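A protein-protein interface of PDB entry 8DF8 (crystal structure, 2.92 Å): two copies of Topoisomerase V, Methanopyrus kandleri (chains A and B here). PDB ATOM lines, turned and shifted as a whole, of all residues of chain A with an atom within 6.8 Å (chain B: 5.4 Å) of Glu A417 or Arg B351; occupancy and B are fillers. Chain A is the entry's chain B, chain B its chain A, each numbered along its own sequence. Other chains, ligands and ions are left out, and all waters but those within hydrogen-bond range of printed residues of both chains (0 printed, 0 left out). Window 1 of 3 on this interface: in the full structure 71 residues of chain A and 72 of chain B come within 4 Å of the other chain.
Among the printed residues, merely in contact across the chains: Thr A414 with Glu B359 (3.6 Å), Glu A417 with Glu B359 (3.6 Å), Val A419 with Glu B359 (3.4 Å) and Arg A458 with Arg B351 (3.4 Å).
The backbone NH (N) of Glu A417 is in hydrogen-bond range of the side-chain hydroxyl (OG) of Ser A462 (3.2 Å). The side-chain hydroxyl (OG1) of Thr B355 sits at hydrogen-bond distance from the backbone carbonyl oxygen (O) of Arg B351 (3.0 Å).
The side-chain hydroxyl (OG1) of Thr B355 lies within hydrogen-bond range of the side-chain carboxylate (OE2) of Glu A417 (3.5 Å). The backbone carbonyl oxygen (O) of Lys A416 sits close to the side-chain carboxylate (OE2) of Glu B359 (3.1 Å). The side-chain carboxylate of Glu A417 lies within salt-bridge range of the guanidinium group of Arg B351, 3.0 Å away. The backbone NH (N) of Gly A418 is in hydrogen-bond range of the side-chain carboxylate (OE1) of Glu B359, at 2.8 Å.
No position is printed for both chains.
Printed residues of chain B that touch a printed residue of chain A: Arg B351, Thr B355 and Glu B359. Of the 14 printed residues of chain A, 6 touch a printed residue of chain B. Along chain A the printed residues that touch a printed residue of chain B span positions 414 to 458. Among the printed residues, Asp or Glu carboxylates within 4 Å of a Lys or Arg side-chain nitrogen of the other chain: Glu A417 with Arg B351 (3.0 Å).
Of the printed residues of chain B, Arg A458 touches Arg B351. Arg B351 touches two residues of chain A. Of the printed residues of chain A, Thr B355 touches Glu A417 (3.5 Å). The nearest residue of chain B that does not touch Glu A417 is Thr B352 (5.2 Å).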
ATOM      1  N   LEU A 413      31.887 -26.143  17.282  1.00  0.00           N
ATOM      2  CA  LEU A 413      31.048 -26.268  16.098  1.00  0.00           C
ATOM      3  C   LEU A 413      29.715 -26.946  16.372  1.00  0.00           C
ATOM      4  O   LEU A 413      28.716 -26.595  15.735  1.00  0.00           O
ATOM      5  CB  LEU A 413      31.784 -27.048  15.003  1.00  0.00           C
ATOM      6  CG  LEU A 413      33.057 -26.405  14.451  1.00  0.00           C
ATOM      7  CD1 LEU A 413      33.589 -27.204  13.271  1.00  0.00           C
ATOM      8  CD2 LEU A 413      32.802 -24.959  14.056  1.00  0.00           C
ATOM      9  N   THR A 414      29.673 -27.905  17.301  1.00  0.00           N
ATOM     10  CA  THR A 414      28.427 -28.611  17.581  1.00  0.00           C
ATOM     11  C   THR A 414      27.405 -27.733  18.293  1.00  0.00           C
ATOM     12  O   THR A 414      26.210 -28.043  18.252  1.00  0.00           O
ATOM     13  CB  THR A 414      28.695 -29.863  18.417  1.00  0.00           C
ATOM     14  OG1 THR A 414      29.419 -29.506  19.602  1.00  0.00           O
ATOM     15  CG2 THR A 414      29.496 -30.880  17.615  1.00  0.00           C
ATOM     16  N   LYS A 415      27.842 -26.651  18.941  1.00  0.00           N
ATOM     17  CA  LYS A 415      26.916 -25.757  19.627  1.00  0.00           C
ATOM     18  C   LYS A 415      26.076 -24.922  18.668  1.00  0.00           C
ATOM     19  O   LYS A 415      25.320 -24.059  19.127  1.00  0.00           O
ATOM     20  CB  LYS A 415      27.674 -24.842  20.592  1.00  0.00           C
ATOM     21  CG  LYS A 415      28.448 -23.710  19.935  1.00  0.00           C
ATOM     22  CD  LYS A 415      29.106 -22.830  20.991  1.00  0.00           C
ATOM     23  CE  LYS A 415      29.534 -21.486  20.421  1.00  0.00           C
ATOM     24  NZ  LYS A 415      30.775 -21.586  19.609  1.00  0.00           N
ATOM     25  N   LYS A 416      26.192 -25.147  17.362  1.00  0.00           N
ATOM     26  CA  LYS A 416      25.387 -24.464  16.361  1.00  0.00           C
ATOM     27  C   LYS A 416      24.335 -25.423  15.820  1.00  0.00           C
ATOM     28  O   LYS A 416      24.597 -26.619  15.657  1.00  0.00           O
ATOM     29  CB  LYS A 416      26.261 -23.944  15.216  1.00  0.00           C
ATOM     30  CG  LYS A 416      27.402 -23.035  15.653  1.00  0.00           C
ATOM     31  CD  LYS A 416      26.889 -21.658  16.050  1.00  0.00           C
ATOM     32  CE  LYS A 416      28.029 -20.716  16.405  1.00  0.00           C
ATOM     33  NZ  LYS A 416      27.547 -19.324  16.639  1.00  0.00           N
ATOM     34  N   GLU A 417      23.146 -24.893  15.546  1.00  0.00           N
ATOM     35  CA  GLU A 417      22.036 -25.729  15.108  1.00  0.00           C
ATOM     36  C   GLU A 417      22.327 -26.331  13.739  1.00  0.00           C
ATOM     37  O   GLU A 417      22.765 -25.632  12.820  1.00  0.00           O
ATOM     38  CB  GLU A 417      20.744 -24.916  15.067  1.00  0.00           C
ATOM     39  CG  GLU A 417      19.510 -25.729  14.716  1.00  0.00           C
ATOM     40  CD  GLU A 417      18.222 -24.975  14.983  1.00  0.00           C
ATOM     41  OE1 GLU A 417      18.296 -23.808  15.423  1.00  0.00           O
ATOM     42  OE2 GLU A 417      17.136 -25.550  14.754  1.00  0.00           O
ATOM     43  N   GLY A 418      22.076 -27.634  13.604  1.00  0.00           N
ATOM     44  CA  GLY A 418      22.287 -28.339  12.358  1.00  0.00           C
ATOM     45  C   GLY A 418      23.663 -28.946  12.186  1.00  0.00           C
ATOM     46  O   GLY A 418      23.883 -29.671  11.207  1.00  0.00           O
ATOM     47  N   VAL A 419      24.586 -28.689  13.106  1.00  0.00           N
ATOM     48  CA  VAL A 419      25.961 -29.169  13.011  1.00  0.00           C
ATOM     49  C   VAL A 419      26.072 -30.407  13.892  1.00  0.00           C
ATOM     50  O   VAL A 419      26.173 -30.307  15.118  1.00  0.00           O
ATOM     51  CB  VAL A 419      26.968 -28.093  13.425  1.00  0.00           C
ATOM     52  CG1 VAL A 419      28.391 -28.613  13.280  1.00  0.00           C
ATOM     53  CG2 VAL A 419      26.766 -26.831  12.605  1.00  0.00           C
ATOM     54  N   GLY A 420      26.058 -31.581  13.267  1.00  0.00           N
ATOM     55  CA  GLY A 420      26.268 -32.817  13.986  1.00  0.00           C
ATOM     56  C   GLY A 420      27.729 -33.004  14.358  1.00  0.00           C
ATOM     57  O   GLY A 420      28.556 -32.094  14.278  1.00  0.00           O
ATOM     58  N   ARG A 458      20.489 -25.277   7.180  1.00  0.00           N
ATOM     59  CA  ARG A 458      20.478 -24.885   8.585  1.00  0.00           C
ATOM     60  C   ARG A 458      21.888 -24.616   9.095  1.00  0.00           C
ATOM     61  O   ARG A 458      22.099 -23.696   9.895  1.00  0.00           O
ATOM     62  CB  ARG A 458      19.784 -25.961   9.422  1.00  0.00           C
ATOM     63  CG  ARG A 458      19.633 -25.606  10.894  1.00  0.00           C
ATOM     64  CD  ARG A 458      18.987 -24.239  11.071  1.00  0.00           C
ATOM     65  NE  ARG A 458      17.729 -24.120  10.343  1.00  0.00           N
ATOM     66  CZ  ARG A 458      17.000 -23.014  10.285  1.00  0.00           C
ATOM     67  NH1 ARG A 458      17.372 -21.907  10.911  1.00  0.00           N
ATOM     68  NH2 ARG A 458      15.872 -23.016   9.582  1.00  0.00           N
ATOM     69  N   VAL A 459      22.868 -25.396   8.633  1.00  0.00           N
ATOM     70  CA  VAL A 459      24.254 -25.174   9.041  1.00  0.00           C
ATOM     71  C   VAL A 459      24.720 -23.793   8.600  1.00  0.00           C
ATOM     72  O   VAL A 459      25.302 -23.031   9.384  1.00  0.00           O
ATOM     73  CB  VAL A 459      25.163 -26.279   8.472  1.00  0.00           C
ATOM     74  CG1 VAL A 459      26.571 -26.145   9.028  1.00  0.00           C
ATOM     75  CG2 VAL A 459      24.585 -27.652   8.771  1.00  0.00           C
ATOM     76  N   LEU A 460      24.468 -23.451   7.334  1.00  0.00           N
ATOM     77  CA  LEU A 460      24.850 -22.140   6.821  1.00  0.00           C
ATOM     78  C   LEU A 460      24.151 -21.027   7.591  1.00  0.00           C
ATOM     79  O   LEU A 460      24.782 -20.043   7.997  1.00  0.00           O
ATOM     80  CB  LEU A 460      24.521 -22.045   5.331  1.00  0.00           C
ATOM     81  CG  LEU A 460      25.210 -23.042   4.399  1.00  0.00           C
ATOM     82  CD1 LEU A 460      24.625 -22.951   2.997  1.00  0.00           C
ATOM     83  CD2 LEU A 460      26.709 -22.804   4.374  1.00  0.00           C
ATOM     84  N   ARG A 461      22.839 -21.168   7.799  1.00  0.00           N
ATOM     85  CA  ARG A 461      22.083 -20.138   8.503  1.00  0.00           C
ATOM     86  C   ARG A 461      22.566 -19.962   9.936  1.00  0.00           C
ATOM     87  O   ARG A 461      22.512 -18.852  10.478  1.00  0.00           O
ATOM     88  CB  ARG A 461      20.593 -20.475   8.473  1.00  0.00           C
ATOM     89  CG  ARG A 461      20.015 -20.489   7.071  1.00  0.00           C
ATOM     90  CD  ARG A 461      18.533 -20.810   7.068  1.00  0.00           C
ATOM     91  NE  ARG A 461      18.069 -21.162   5.732  1.00  0.00           N
ATOM     92  CZ  ARG A 461      16.802 -21.118   5.343  1.00  0.00           C
ATOM     93  NH1 ARG A 461      15.842 -20.722   6.162  1.00  0.00           N
ATOM     94  NH2 ARG A 461      16.492 -21.475   4.100  1.00  0.00           N
ATOM     95  N   SER A 462      23.040 -21.039  10.567  1.00  0.00           N
ATOM     96  CA  SER A 462      23.563 -20.928  11.921  1.00  0.00           C
ATOM     97  C   SER A 462      24.981 -20.373  11.943  1.00  0.00           C
ATOM     98  O   SER A 462      25.397 -19.794  12.952  1.00  0.00           O
ATOM     99  CB  SER A 462      23.520 -22.289  12.615  1.00  0.00           C
ATOM    100  OG  SER A 462      23.915 -22.177  13.970  1.00  0.00           O
ATOM    101  N   LEU A 463      25.732 -20.538  10.852  1.00  0.00           N
ATOM    102  CA  LEU A 463      27.132 -20.130  10.802  1.00  0.00           C
ATOM    103  C   LEU A 463      27.336 -18.754  10.177  1.00  0.00           C
ATOM    104  O   LEU A 463      28.097 -17.942  10.713  1.00  0.00           O
ATOM    105  CB  LEU A 463      27.953 -21.173  10.033  1.00  0.00           C
ATOM    106  CG  LEU A 463      28.378 -22.415  10.817  1.00  0.00           C
ATOM    107  CD1 LEU A 463      28.953 -23.469   9.890  1.00  0.00           C
ATOM    108  CD2 LEU A 463      29.393 -22.037  11.887  1.00  0.00           C
ATOM    109  N   TYR B 305      11.688 -22.377   3.732  1.00  0.00           N
ATOM    110  CA  TYR B 305      12.074 -23.755   3.995  1.00  0.00           C
ATOM    111  C   TYR B 305      12.202 -24.608   2.740  1.00  0.00           C
ATOM    112  O   TYR B 305      12.533 -25.795   2.849  1.00  0.00           O
ATOM    113  CB  TYR B 305      11.075 -24.406   4.961  1.00  0.00           C
ATOM    114  CG  TYR B 305      10.850 -23.602   6.223  1.00  0.00           C
ATOM    115  CD1 TYR B 305      11.875 -23.417   7.143  1.00  0.00           C
ATOM    116  CD2 TYR B 305       9.617 -23.022   6.491  1.00  0.00           C
ATOM    117  CE1 TYR B 305      11.678 -22.680   8.297  1.00  0.00           C
ATOM    118  CE2 TYR B 305       9.409 -22.284   7.642  1.00  0.00           C
ATOM    119  CZ  TYR B 305      10.443 -22.117   8.541  1.00  0.00           C
ATOM    120  OH  TYR B 305      10.241 -21.383   9.688  1.00  0.00           O
ATOM    121  N   ALA B 327       5.760 -26.691  13.304  1.00  0.00           N
ATOM    122  CA  ALA B 327       7.087 -26.864  13.882  1.00  0.00           C
ATOM    123  C   ALA B 327       7.069 -27.673  15.172  1.00  0.00           C
ATOM    124  O   ALA B 327       8.141 -27.995  15.695  1.00  0.00           O
ATOM    125  CB  ALA B 327       7.730 -25.499  14.140  1.00  0.00           C
ATOM    126  N   ALA B 346      10.214 -32.241   6.184  1.00  0.00           N
ATOM    127  CA  ALA B 346       9.735 -32.211   7.562  1.00  0.00           C
ATOM    128  C   ALA B 346      10.817 -31.716   8.512  1.00  0.00           C
ATOM    129  O   ALA B 346      10.535 -30.954   9.445  1.00  0.00           O
ATOM    130  CB  ALA B 346       9.245 -33.597   7.979  1.00  0.00           C
ATOM    131  N   LYS B 347      12.064 -32.145   8.297  1.00  0.00           N
ATOM    132  CA  LYS B 347      13.162 -31.649   9.119  1.00  0.00           C
ATOM    133  C   LYS B 347      13.393 -30.160   8.902  1.00  0.00           C
ATOM    134  O   LYS B 347      13.745 -29.443   9.846  1.00  0.00           O
ATOM    135  CB  LYS B 347      14.436 -32.439   8.823  1.00  0.00           C
ATOM    136  CG  LYS B 347      14.394 -33.880   9.305  1.00  0.00           C
ATOM    137  CD  LYS B 347      15.320 -34.773   8.492  1.00  0.00           C
ATOM    138  CE  LYS B 347      16.778 -34.393   8.690  1.00  0.00           C
ATOM    139  NZ  LYS B 347      17.697 -35.334   7.992  1.00  0.00           N
ATOM    140  N   SER B 348      13.189 -29.676   7.676  1.00  0.00           N
ATOM    141  CA  SER B 348      13.391 -28.257   7.402  1.00  0.00           C
ATOM    142  C   SER B 348      12.318 -27.406   8.069  1.00  0.00           C
ATOM    143  O   SER B 348      12.613 -26.318   8.578  1.00  0.00           O
ATOM    144  CB  SER B 348      13.413 -28.012   5.894  1.00  0.00           C
ATOM    145  OG  SER B 348      12.118 -28.153   5.337  1.00  0.00           O
ATOM    146  N   VAL B 349      11.070 -27.881   8.086  1.00  0.00           N
ATOM    147  CA  VAL B 349      10.006 -27.083   8.690  1.00  0.00           C
ATOM    148  C   VAL B 349       9.985 -27.253  10.208  1.00  0.00           C
ATOM    149  O   VAL B 349       9.834 -26.275  10.949  1.00  0.00           O
ATOM    150  CB  VAL B 349       8.643 -27.420   8.053  1.00  0.00           C
ATOM    151  CG1 VAL B 349       8.331 -28.900   8.161  1.00  0.00           C
ATOM    152  CG2 VAL B 349       7.542 -26.592   8.696  1.00  0.00           C
ATOM    153  N   ASN B 350      10.147 -28.480  10.698  1.00  0.00           N
ATOM    154  CA  ASN B 350      10.205 -28.742  12.136  1.00  0.00           C
ATOM    155  C   ASN B 350      11.672 -28.729  12.545  1.00  0.00           C
ATOM    156  O   ASN B 350      12.382 -29.726  12.392  1.00  0.00           O
ATOM    157  CB  ASN B 350       9.531 -30.069  12.471  1.00  0.00           C
ATOM    158  CG  ASN B 350       9.334 -30.268  13.964  1.00  0.00           C
ATOM    159  OD1 ASN B 350      10.178 -29.885  14.777  1.00  0.00           O
ATOM    160  ND2 ASN B 350       8.207 -30.866  14.334  1.00  0.00           N
ATOM    161  N   ARG B 351      12.132 -27.591  13.072  1.00  0.00           N
ATOM    162  CA  ARG B 351      13.540 -27.463  13.434  1.00  0.00           C
ATOM    163  C   ARG B 351      13.926 -28.413  14.560  1.00  0.00           C
ATOM    164  O   ARG B 351      15.060 -28.905  14.594  1.00  0.00           O
ATOM    165  CB  ARG B 351      13.852 -26.020  13.827  1.00  0.00           C
ATOM    166  CG  ARG B 351      13.390 -24.988  12.814  1.00  0.00           C
ATOM    167  CD  ARG B 351      14.514 -24.029  12.476  1.00  0.00           C
ATOM    168  NE  ARG B 351      15.163 -23.504  13.672  1.00  0.00           N
ATOM    169  CZ  ARG B 351      15.015 -22.267  14.123  1.00  0.00           C
ATOM    170  NH1 ARG B 351      14.253 -21.388  13.494  1.00  0.00           N
ATOM    171  NH2 ARG B 351      15.650 -21.900  15.233  1.00  0.00           N
ATOM    172  N   THR B 352      13.002 -28.686  15.484  1.00  0.00           N
ATOM    173  CA  THR B 352      13.287 -29.631  16.560  1.00  0.00           C
ATOM    174  C   THR B 352      13.486 -31.041  16.016  1.00  0.00           C
ATOM    175  O   THR B 352      14.390 -31.761  16.457  1.00  0.00           O
ATOM    176  CB  THR B 352      12.165 -29.595  17.598  1.00  0.00           C
ATOM    177  OG1 THR B 352      12.207 -28.345  18.303  1.00  0.00           O
ATOM    178  CG2 THR B 352      12.310 -30.736  18.591  1.00  0.00           C
ATOM    179  N   LEU B 353      12.648 -31.452  15.060  1.00  0.00           N
ATOM    180  CA  LEU B 353      12.820 -32.761  14.434  1.00  0.00           C
ATOM    181  C   LEU B 353      14.186 -32.879  13.768  1.00  0.00           C
ATOM    182  O   LEU B 353      14.851 -33.916  13.877  1.00  0.00           O
ATOM    183  CB  LEU B 353      11.706 -33.005  13.416  1.00  0.00           C
ATOM    184  CG  LEU B 353      11.782 -34.308  12.619  1.00  0.00           C
ATOM    185  CD1 LEU B 353      11.471 -35.495  13.511  1.00  0.00           C
ATOM    186  CD2 LEU B 353      10.839 -34.271  11.428  1.00  0.00           C
ATOM    187  N   ALA B 354      14.617 -31.825  13.069  1.00  0.00           N
ATOM    188  CA  ALA B 354      15.932 -31.839  12.436  1.00  0.00           C
ATOM    189  C   ALA B 354      17.040 -31.936  13.476  1.00  0.00           C
ATOM    190  O   ALA B 354      17.963 -32.747  13.343  1.00  0.00           O
ATOM    191  CB  ALA B 354      16.114 -30.591  11.572  1.00  0.00           C
ATOM    192  N   THR B 355      16.972 -31.101  14.518  1.00  0.00           N
ATOM    193  CA  THR B 355      17.990 -31.142  15.563  1.00  0.00           C
ATOM    194  C   THR B 355      18.063 -32.515  16.220  1.00  0.00           C
ATOM    195  O   THR B 355      19.151 -32.974  16.586  1.00  0.00           O
ATOM    196  CB  THR B 355      17.710 -30.064  16.614  1.00  0.00           C
ATOM    197  OG1 THR B 355      17.678 -28.776  15.984  1.00  0.00           O
ATOM    198  CG2 THR B 355      18.788 -30.065  17.692  1.00  0.00           C
ATOM    199  N   LEU B 356      16.924 -33.193  16.361  1.00  0.00           N
ATOM    200  CA  LEU B 356      16.932 -34.522  16.962  1.00  0.00           C
ATOM    201  C   LEU B 356      17.532 -35.555  16.015  1.00  0.00           C
ATOM    202  O   LEU B 356      18.409 -36.334  16.406  1.00  0.00           O
ATOM    203  CB  LEU B 356      15.512 -34.920  17.369  1.00  0.00           C
ATOM    204  CG  LEU B 356      14.924 -34.158  18.559  1.00  0.00           C
ATOM    205  CD1 LEU B 356      13.540 -34.684  18.899  1.00  0.00           C
ATOM    206  CD2 LEU B 356      15.847 -34.226  19.768  1.00  0.00           C
ATOM    207  N   GLU B 359      21.612 -33.751  14.627  1.00  0.00           N
ATOM    208  CA  GLU B 359      22.594 -33.464  15.668  1.00  0.00           C
ATOM    209  C   GLU B 359      22.655 -34.543  16.744  1.00  0.00           C
ATOM    210  O   GLU B 359      23.643 -34.600  17.483  1.00  0.00           O
ATOM    211  CB  GLU B 359      22.290 -32.114  16.319  1.00  0.00           C
ATOM    212  CG  GLU B 359      22.853 -30.917  15.577  1.00  0.00           C
ATOM    213  CD  GLU B 359      22.308 -29.604  16.103  1.00  0.00           C
ATOM    214  OE1 GLU B 359      21.191 -29.218  15.695  1.00  0.00           O
ATOM    215  OE2 GLU B 359      22.991 -28.963  16.931  1.00  0.00           O
